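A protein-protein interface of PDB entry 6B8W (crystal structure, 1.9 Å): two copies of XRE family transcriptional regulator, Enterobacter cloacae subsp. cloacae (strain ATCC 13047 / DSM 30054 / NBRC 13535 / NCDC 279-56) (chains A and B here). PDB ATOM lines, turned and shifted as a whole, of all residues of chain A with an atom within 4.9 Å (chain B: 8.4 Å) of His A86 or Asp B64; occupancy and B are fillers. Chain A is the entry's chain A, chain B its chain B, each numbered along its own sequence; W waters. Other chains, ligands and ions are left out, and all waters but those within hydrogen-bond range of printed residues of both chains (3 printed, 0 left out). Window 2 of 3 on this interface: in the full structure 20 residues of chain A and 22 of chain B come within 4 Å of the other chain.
N of Ser A21 is in hydrogen-bond range of O of Lys A6, 2.7 Å away.
A ring nitrogen (NE2) of His A86 sits at hydrogen-bond distance from the side-chain hydroxyl (OG) of Ser A21 (2.7 Å).
The backbone carbonyl oxygen of Val B45 lies within hydrogen-bond range of the backbone NH of Asp B64 (3.3 Å).
O of His A86 lies within hydrogen-bond range of N of Ile A46 (2.8 Å).
N of Ile B46 lies within hydrogen-bond range of O of His B86, at 2.8 Å.
N of His A86 is in hydrogen-bond range of O of Ser A47 (2.9 Å).
Lys A6 touches Asp B64.
O of Asp B64 touches CD2 of Leu A8 (3.4 Å).
Ile A46 touches Ile B46.
His A86 touches Asp B64.
Of the printed residues of chain B, Lys A6 touches Asp B64 (3.7 Å).
Of the printed residues of chain B, Leu A8 touches Asp B64 (3.4 Å).
Printed residues of chain B within 4 Å of Ile A46: Ile B46.
No residue of chain B comes within 4 Å of Val A85.
Of the printed residues of chain B, His A86 touches Asp B64.
Val B43 touches none of the printed residues of chain A.
Printed residues of chain A within 4 Å of Ile B46: Ile A46 (3.5 Å).
Asp B64 touches just these residues of chain A: Lys A6, Leu A8 and His A86.
Gly B66 touches none of the printed residues of chain A.
The nearest printed residue of chain B that does not touch Leu A8 is Val B44 (4.2 Å).
Hydrophobic or aromatic side chains of chain B within 4 Å of the printed part of chain A: Ile B46.
Printed residues of chain A that touch a printed residue of chain B: Lys A6, Leu A8, Ile A46 and His A86.
Hydrophobic or aromatic side chains of chain A within 4 Å of the printed part of chain B: Leu A8, Ile A46 and His A86.
Ile B46 touches its own counterpart, Ile A46.
Of the 4 pairs that touch across the chains among the printed residues, 1 has its exchanged pair printed and touching as well.
Water W1 lies within hydrogen-bond range of OD1 of Asp B64 (2.6 Å) and OG of Ser A21 (2.7 Å).
Water W2 lies within hydrogen-bond range of O of Leu A8, O of Asp B64 and N of Gly B66.
Water W3 lies within hydrogen-bond range of NE2 of His A88 (2.9 Å), OD1 of Asp B64 (3.0 Å), NE2 of His A86 (3.3 Å) and OG of Ser A21 (3.5 Å).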
ATOM      1  N   LYS A   6      22.059  -5.427  22.930  1.00  0.00           N
ATOM      2  CA  LYS A   6      20.873  -4.760  22.418  1.00  0.00           C
ATOM      3  C   LYS A   6      20.134  -5.697  21.435  1.00  0.00           C
ATOM      4  O   LYS A   6      20.735  -6.181  20.478  1.00  0.00           O
ATOM      5  CB  LYS A   6      21.336  -3.478  21.706  1.00  0.00           C
ATOM      6  CG  LYS A   6      20.455  -2.981  20.583  1.00  0.00           C
ATOM      7  CD  LYS A   6      21.100  -1.817  19.835  1.00  0.00           C
ATOM      8  CE  LYS A   6      20.417  -1.586  18.488  1.00  0.00           C
ATOM      9  NZ  LYS A   6      18.931  -1.537  18.600  1.00  0.00           N
ATOM     10  N   LEU A   8      18.178  -6.526  18.223  1.00  0.00           N
ATOM     11  CA  LEU A   8      17.945  -5.784  16.970  1.00  0.00           C
ATOM     12  C   LEU A   8      16.470  -5.790  16.603  1.00  0.00           C
ATOM     13  O   LEU A   8      15.969  -4.887  15.960  1.00  0.00           O
ATOM     14  CB  LEU A   8      18.790  -6.345  15.823  1.00  0.00           C
ATOM     15  CG  LEU A   8      20.240  -5.875  15.807  1.00  0.00           C
ATOM     16  CD1 LEU A   8      21.114  -6.781  14.955  1.00  0.00           C
ATOM     17  CD2 LEU A   8      20.331  -4.435  15.321  1.00  0.00           C
ATOM     18  N   SER A  21      22.592  -7.536  19.047  1.00  0.00           N
ATOM     19  CA  SER A  21      23.722  -6.738  18.637  1.00  0.00           C
ATOM     20  C   SER A  21      24.541  -6.534  19.915  1.00  0.00           C
ATOM     21  O   SER A  21      24.032  -5.970  20.903  1.00  0.00           O
ATOM     22  CB  SER A  21      23.252  -5.405  18.075  1.00  0.00           C
ATOM     23  OG  SER A  21      24.368  -4.594  17.809  1.00  0.00           O
ATOM     24  N   ILE A  22      25.807  -6.935  19.868  1.00  0.00           N
ATOM     25  CA  ILE A  22      26.671  -6.924  21.046  1.00  0.00           C
ATOM     26  C   ILE A  22      27.962  -6.166  20.796  1.00  0.00           C
ATOM     27  O   ILE A  22      28.599  -6.349  19.766  1.00  0.00           O
ATOM     28  CB  ILE A  22      27.012  -8.375  21.431  1.00  0.00           C
ATOM     29  CG1 ILE A  22      25.713  -9.168  21.686  1.00  0.00           C
ATOM     30  CG2 ILE A  22      27.960  -8.427  22.634  1.00  0.00           C
ATOM     31  CD1 ILE A  22      25.920 -10.640  21.967  1.00  0.00           C
ATOM     32  N   ILE A  23      28.339  -5.315  21.745  1.00  0.00           N
ATOM     33  CA  ILE A  23      29.597  -4.577  21.671  1.00  0.00           C
ATOM     34  C   ILE A  23      30.428  -5.046  22.884  1.00  0.00           C
ATOM     35  O   ILE A  23      29.989  -4.926  24.028  1.00  0.00           O
ATOM     36  CB  ILE A  23      29.410  -3.078  21.672  1.00  0.00           C
ATOM     37  CG1 ILE A  23      28.585  -2.668  20.430  1.00  0.00           C
ATOM     38  CG2 ILE A  23      30.774  -2.393  21.655  1.00  0.00           C
ATOM     39  CD1 ILE A  23      28.211  -1.202  20.361  1.00  0.00           C
ATOM     40  N   VAL A  44      28.247 -13.244  13.730  1.00  0.00           N
ATOM     41  CA  VAL A  44      28.769 -12.531  12.568  1.00  0.00           C
ATOM     42  C   VAL A  44      29.409 -11.257  13.092  1.00  0.00           C
ATOM     43  O   VAL A  44      28.780 -10.507  13.844  1.00  0.00           O
ATOM     44  CB  VAL A  44      27.664 -12.148  11.561  1.00  0.00           C
ATOM     45  CG1 VAL A  44      28.242 -11.325  10.411  1.00  0.00           C
ATOM     46  CG2 VAL A  44      26.967 -13.391  11.033  1.00  0.00           C
ATOM     47  N   VAL A  45      30.664 -11.019  12.732  1.00  0.00           N
ATOM     48  CA  VAL A  45      31.355  -9.796  13.164  1.00  0.00           C
ATOM     49  C   VAL A  45      30.949  -8.644  12.251  1.00  0.00           C
ATOM     50  O   VAL A  45      30.925  -8.791  11.039  1.00  0.00           O
ATOM     51  CB  VAL A  45      32.884  -9.991  13.166  1.00  0.00           C
ATOM     52  CG1 VAL A  45      33.625  -8.703  13.506  1.00  0.00           C
ATOM     53  CG2 VAL A  45      33.261 -11.074  14.177  1.00  0.00           C
ATOM     54  N   ILE A  46      30.631  -7.505  12.852  1.00  0.00           N
ATOM     55  CA  ILE A  46      30.217  -6.316  12.116  1.00  0.00           C
ATOM     56  C   ILE A  46      31.409  -5.384  11.978  1.00  0.00           C
ATOM     57  O   ILE A  46      31.743  -4.981  10.870  1.00  0.00           O
ATOM     58  CB  ILE A  46      29.041  -5.604  12.818  1.00  0.00           C
ATOM     59  CG1 ILE A  46      27.885  -6.587  13.059  1.00  0.00           C
ATOM     60  CG2 ILE A  46      28.590  -4.399  12.019  1.00  0.00           C
ATOM     61  CD1 ILE A  46      27.440  -7.385  11.859  1.00  0.00           C
ATOM     62  N   SER A  47      32.040  -5.049  13.105  1.00  0.00           N
ATOM     63  CA  SER A  47      33.242  -4.189  13.095  1.00  0.00           C
ATOM     64  C   SER A  47      34.209  -4.643  14.193  1.00  0.00           C
ATOM     65  O   SER A  47      33.793  -5.139  15.225  1.00  0.00           O
ATOM     66  CB  SER A  47      32.873  -2.719  13.265  1.00  0.00           C
ATOM     67  OG  SER A  47      32.272  -2.469  14.512  1.00  0.00           O
ATOM     68  N   PRO A  84      36.695  -1.510  20.607  1.00  0.00           N
ATOM     69  CA  PRO A  84      35.486  -2.350  20.734  1.00  0.00           C
ATOM     70  C   PRO A  84      35.228  -3.236  19.521  1.00  0.00           C
ATOM     71  O   PRO A  84      35.612  -2.883  18.400  1.00  0.00           O
ATOM     72  CB  PRO A  84      34.350  -1.336  20.872  1.00  0.00           C
ATOM     73  CG  PRO A  84      35.000  -0.074  21.361  1.00  0.00           C
ATOM     74  CD  PRO A  84      36.396  -0.071  20.808  1.00  0.00           C
ATOM     75  N   VAL A  85      34.637  -4.396  19.761  1.00  0.00           N
ATOM     76  CA  VAL A  85      34.228  -5.271  18.656  1.00  0.00           C
ATOM     77  C   VAL A  85      32.712  -5.352  18.701  1.00  0.00           C
ATOM     78  O   VAL A  85      32.130  -5.562  19.764  1.00  0.00           O
ATOM     79  CB  VAL A  85      34.858  -6.670  18.686  1.00  0.00           C
ATOM     80  CG1 VAL A  85      34.550  -7.412  19.983  1.00  0.00           C
ATOM     81  CG2 VAL A  85      34.406  -7.494  17.483  1.00  0.00           C
ATOM     82  N   HIS A  86      32.088  -5.121  17.542  1.00  0.00           N
ATOM     83  CA  HIS A  86      30.650  -5.161  17.390  1.00  0.00           C
ATOM     84  C   HIS A  86      30.296  -6.417  16.602  1.00  0.00           C
ATOM     85  O   HIS A  86      30.811  -6.624  15.512  1.00  0.00           O
ATOM     86  CB  HIS A  86      30.186  -3.908  16.636  1.00  0.00           C
ATOM     87  CG  HIS A  86      28.708  -3.849  16.389  1.00  0.00           C
ATOM     88  ND1 HIS A  86      28.163  -3.093  15.374  1.00  0.00           N
ATOM     89  CD2 HIS A  86      27.670  -4.486  16.983  1.00  0.00           C
ATOM     90  CE1 HIS A  86      26.848  -3.227  15.382  1.00  0.00           C
ATOM     91  NE2 HIS A  86      26.524  -4.089  16.336  1.00  0.00           N
ATOM     92  N   PHE A  87      29.453  -7.275  17.167  1.00  0.00           N
ATOM     93  CA  PHE A  87      29.044  -8.471  16.449  1.00  0.00           C
ATOM     94  C   PHE A  87      27.574  -8.728  16.673  1.00  0.00           C
ATOM     95  O   PHE A  87      26.954  -8.108  17.524  1.00  0.00           O
ATOM     96  CB  PHE A  87      29.900  -9.687  16.819  1.00  0.00           C
ATOM     97  CG  PHE A  87      29.807 -10.107  18.262  1.00  0.00           C
ATOM     98  CD1 PHE A  87      30.595  -9.500  19.228  1.00  0.00           C
ATOM     99  CD2 PHE A  87      28.961 -11.137  18.643  1.00  0.00           C
ATOM    100  CE1 PHE A  87      30.526  -9.899  20.549  1.00  0.00           C
ATOM    101  CE2 PHE A  87      28.881 -11.550  19.966  1.00  0.00           C
ATOM    102  CZ  PHE A  87      29.670 -10.937  20.928  1.00  0.00           C
ATOM    103  N   HIS A  88      26.996  -9.571  15.828  1.00  0.00           N
ATOM    104  CA  HIS A  88      25.620  -9.992  16.025  1.00  0.00           C
ATOM    105  C   HIS A  88      25.616 -11.434  16.442  1.00  0.00           C
ATOM    106  O   HIS A  88      26.448 -12.231  15.982  1.00  0.00           O
ATOM    107  CB  HIS A  88      24.734  -9.906  14.779  1.00  0.00           C
ATOM    108  CG  HIS A  88      24.504  -8.529  14.263  1.00  0.00           C
ATOM    109  ND1 HIS A  88      23.909  -8.299  13.038  1.00  0.00           N
ATOM    110  CD2 HIS A  88      24.819  -7.314  14.764  1.00  0.00           C
ATOM    111  CE1 HIS A  88      23.844  -7.000  12.823  1.00  0.00           C
ATOM    112  NE2 HIS A  88      24.402  -6.378  13.845  1.00  0.00           N
ATOM    113  N   VAL B  43      16.239  -6.714   7.403  1.00  0.00           N
ATOM    114  CA  VAL B  43      17.324  -5.941   6.853  1.00  0.00           C
ATOM    115  C   VAL B  43      17.882  -5.119   7.995  1.00  0.00           C
ATOM    116  O   VAL B  43      17.118  -4.602   8.816  1.00  0.00           O
ATOM    117  CB  VAL B  43      16.861  -5.023   5.692  1.00  0.00           C
ATOM    118  CG1 VAL B  43      17.888  -3.932   5.409  1.00  0.00           C
ATOM    119  CG2 VAL B  43      16.586  -5.847   4.437  1.00  0.00           C
ATOM    120  N   VAL B  44      19.213  -5.065   8.085  1.00  0.00           N
ATOM    121  CA  VAL B  44      19.909  -4.277   9.092  1.00  0.00           C
ATOM    122  C   VAL B  44      21.005  -3.512   8.379  1.00  0.00           C
ATOM    123  O   VAL B  44      21.804  -4.114   7.644  1.00  0.00           O
ATOM    124  CB  VAL B  44      20.643  -5.145  10.160  1.00  0.00           C
ATOM    125  CG1 VAL B  44      21.220  -4.237  11.248  1.00  0.00           C
ATOM    126  CG2 VAL B  44      19.708  -6.151  10.767  1.00  0.00           C
ATOM    127  N   VAL B  45      21.097  -2.219   8.647  1.00  0.00           N
ATOM    128  CA  VAL B  45      22.136  -1.383   8.046  1.00  0.00           C
ATOM    129  C   VAL B  45      23.394  -1.489   8.897  1.00  0.00           C
ATOM    130  O   VAL B  45      23.334  -1.399  10.122  1.00  0.00           O
ATOM    131  CB  VAL B  45      21.673   0.078   7.916  1.00  0.00           C
ATOM    132  CG1 VAL B  45      22.765   0.968   7.337  1.00  0.00           C
ATOM    133  CG2 VAL B  45      20.428   0.143   7.023  1.00  0.00           C
ATOM    134  N   ILE B  46      24.528  -1.713   8.236  1.00  0.00           N
ATOM    135  CA  ILE B  46      25.818  -1.838   8.919  1.00  0.00           C
ATOM    136  C   ILE B  46      26.496  -0.485   8.933  1.00  0.00           C
ATOM    137  O   ILE B  46      26.918  -0.025   9.972  1.00  0.00           O
ATOM    138  CB  ILE B  46      26.731  -2.870   8.223  1.00  0.00           C
ATOM    139  CG1 ILE B  46      26.038  -4.242   8.163  1.00  0.00           C
ATOM    140  CG2 ILE B  46      28.084  -2.897   8.910  1.00  0.00           C
ATOM    141  CD1 ILE B  46      25.357  -4.671   9.450  1.00  0.00           C
ATOM    142  N   SER B  47      26.612   0.131   7.761  1.00  0.00           N
ATOM    143  CA  SER B  47      27.177   1.483   7.649  1.00  0.00           C
ATOM    144  C   SER B  47      26.481   2.190   6.490  1.00  0.00           C
ATOM    145  O   SER B  47      25.941   1.547   5.561  1.00  0.00           O
ATOM    146  CB  SER B  47      28.690   1.478   7.433  1.00  0.00           C
ATOM    147  OG  SER B  47      29.014   0.968   6.151  1.00  0.00           O
ATOM    148  N   GLY B  48      26.494   3.514   6.534  1.00  0.00           N
ATOM    149  CA  GLY B  48      25.842   4.299   5.493  1.00  0.00           C
ATOM    150  C   GLY B  48      24.358   4.500   5.781  1.00  0.00           C
ATOM    151  O   GLY B  48      23.918   4.392   6.930  1.00  0.00           O
ATOM    152  N   LEU B  61      16.773   4.013   6.377  1.00  0.00           N
ATOM    153  CA  LEU B  61      17.293   3.225   7.522  1.00  0.00           C
ATOM    154  C   LEU B  61      18.778   3.554   7.788  1.00  0.00           C
ATOM    155  O   LEU B  61      19.569   3.715   6.842  1.00  0.00           O
ATOM    156  CB  LEU B  61      17.129   1.737   7.215  1.00  0.00           C
ATOM    157  CG  LEU B  61      15.683   1.264   7.054  1.00  0.00           C
ATOM    158  CD1 LEU B  61      15.600  -0.094   6.369  1.00  0.00           C
ATOM    159  CD2 LEU B  61      14.999   1.230   8.416  1.00  0.00           C
ATOM    160  N   TYR B  62      19.151   3.611   9.073  1.00  0.00           N
ATOM    161  CA  TYR B  62      20.513   3.957   9.505  1.00  0.00           C
ATOM    162  C   TYR B  62      21.145   2.811  10.306  1.00  0.00           C
ATOM    163  O   TYR B  62      20.437   1.901  10.719  1.00  0.00           O
ATOM    164  CB  TYR B  62      20.473   5.235  10.350  1.00  0.00           C
ATOM    165  CG  TYR B  62      19.877   6.421   9.618  1.00  0.00           C
ATOM    166  CD1 TYR B  62      18.506   6.651   9.637  1.00  0.00           C
ATOM    167  CD2 TYR B  62      20.683   7.307   8.895  1.00  0.00           C
ATOM    168  CE1 TYR B  62      17.944   7.731   8.972  1.00  0.00           C
ATOM    169  CE2 TYR B  62      20.126   8.396   8.222  1.00  0.00           C
ATOM    170  CZ  TYR B  62      18.756   8.600   8.269  1.00  0.00           C
ATOM    171  OH  TYR B  62      18.180   9.654   7.612  1.00  0.00           O
ATOM    172  N   PRO B  63      22.477   2.864  10.543  1.00  0.00           N
ATOM    173  CA  PRO B  63      23.124   1.777  11.272  1.00  0.00           C
ATOM    174  C   PRO B  63      22.464   1.437  12.587  1.00  0.00           C
ATOM    175  O   PRO B  63      21.900   2.308  13.254  1.00  0.00           O
ATOM    176  CB  PRO B  63      24.546   2.295  11.491  1.00  0.00           C
ATOM    177  CG  PRO B  63      24.766   3.155  10.308  1.00  0.00           C
ATOM    178  CD  PRO B  63      23.464   3.877  10.150  1.00  0.00           C
ATOM    179  N   ASP B  64      22.502   0.151  12.904  1.00  0.00           N
ATOM    180  CA  ASP B  64      21.904  -0.423  14.104  1.00  0.00           C
ATOM    181  C   ASP B  64      20.382  -0.507  13.995  1.00  0.00           C
ATOM    182  O   ASP B  64      19.742  -1.137  14.842  1.00  0.00           O
ATOM    183  CB  ASP B  64      22.333   0.317  15.387  1.00  0.00           C
ATOM    184  CG  ASP B  64      23.842   0.289  15.603  1.00  0.00           C
ATOM    185  OD1 ASP B  64      24.452  -0.783  15.407  1.00  0.00           O
ATOM    186  OD2 ASP B  64      24.413   1.330  15.995  1.00  0.00           O
ATOM    187  N   GLN B  65      19.808   0.100  12.956  1.00  0.00           N
ATOM    188  CA  GLN B  65      18.363   0.055  12.753  1.00  0.00           C
ATOM    189  C   GLN B  65      18.083  -1.017  11.720  1.00  0.00           C
ATOM    190  O   GLN B  65      18.920  -1.295  10.817  1.00  0.00           O
ATOM    191  CB  GLN B  65      17.822   1.369  12.220  1.00  0.00           C
ATOM    192  CG  GLN B  65      18.195   2.582  13.040  1.00  0.00           C
ATOM    193  CD  GLN B  65      17.583   3.848  12.489  1.00  0.00           C
ATOM    194  OE1 GLN B  65      17.128   3.892  11.330  1.00  0.00           O
ATOM    195  NE2 GLN B  65      17.579   4.896  13.302  1.00  0.00           N
ATOM    196  N   GLY B  66      16.899  -1.598  11.837  1.00  0.00           N
ATOM    197  CA  GLY B  66      16.501  -2.639  10.927  1.00  0.00           C
ATOM    198  C   GLY B  66      15.011  -2.712  10.774  1.00  0.00           C
ATOM    199  O   GLY B  66      14.264  -1.977  11.421  1.00  0.00           O
ATOM    200  N   VAL B  67      14.578  -3.601   9.906  1.00  0.00           N
ATOM    201  CA  VAL B  67      13.170  -3.777   9.678  1.00  0.00           C
ATOM    202  C   VAL B  67      12.912  -5.230   9.319  1.00  0.00           C
ATOM    203  O   VAL B  67      13.750  -5.880   8.700  1.00  0.00           O
ATOM    204  CB  VAL B  67      12.652  -2.801   8.588  1.00  0.00           C
ATOM    205  CG1 VAL B  67      13.434  -2.958   7.295  1.00  0.00           C
ATOM    206  CG2 VAL B  67      11.160  -2.999   8.355  1.00  0.00           C
ATOM    207  N   HIS B  86      26.199  -0.345   3.309  1.00  0.00           N
ATOM    208  CA  HIS B  86      26.445  -1.751   3.557  1.00  0.00           C
ATOM    209  C   HIS B  86      25.355  -2.251   4.505  1.00  0.00           C
ATOM    210  O   HIS B  86      25.132  -1.658   5.544  1.00  0.00           O
ATOM    211  CB  HIS B  86      27.868  -1.899   4.151  1.00  0.00           C
ATOM    212  CG  HIS B  86      28.238  -3.290   4.562  1.00  0.00           C
ATOM    213  ND1 HIS B  86      29.131  -3.542   5.584  1.00  0.00           N
ATOM    214  CD2 HIS B  86      27.800  -4.502   4.137  1.00  0.00           C
ATOM    215  CE1 HIS B  86      29.258  -4.851   5.740  1.00  0.00           C
ATOM    216  NE2 HIS B  86      28.462  -5.457   4.880  1.00  0.00           N
HETATM  217  O   HOH W   1      23.101  -2.454  16.831  1.00  0.00           O
HETATM  218  O   HOH W   2      17.493  -2.966  14.920  1.00  0.00           O
HETATM  219  O   HOH W   3      23.794  -3.587  14.520  1.00  0.00           O
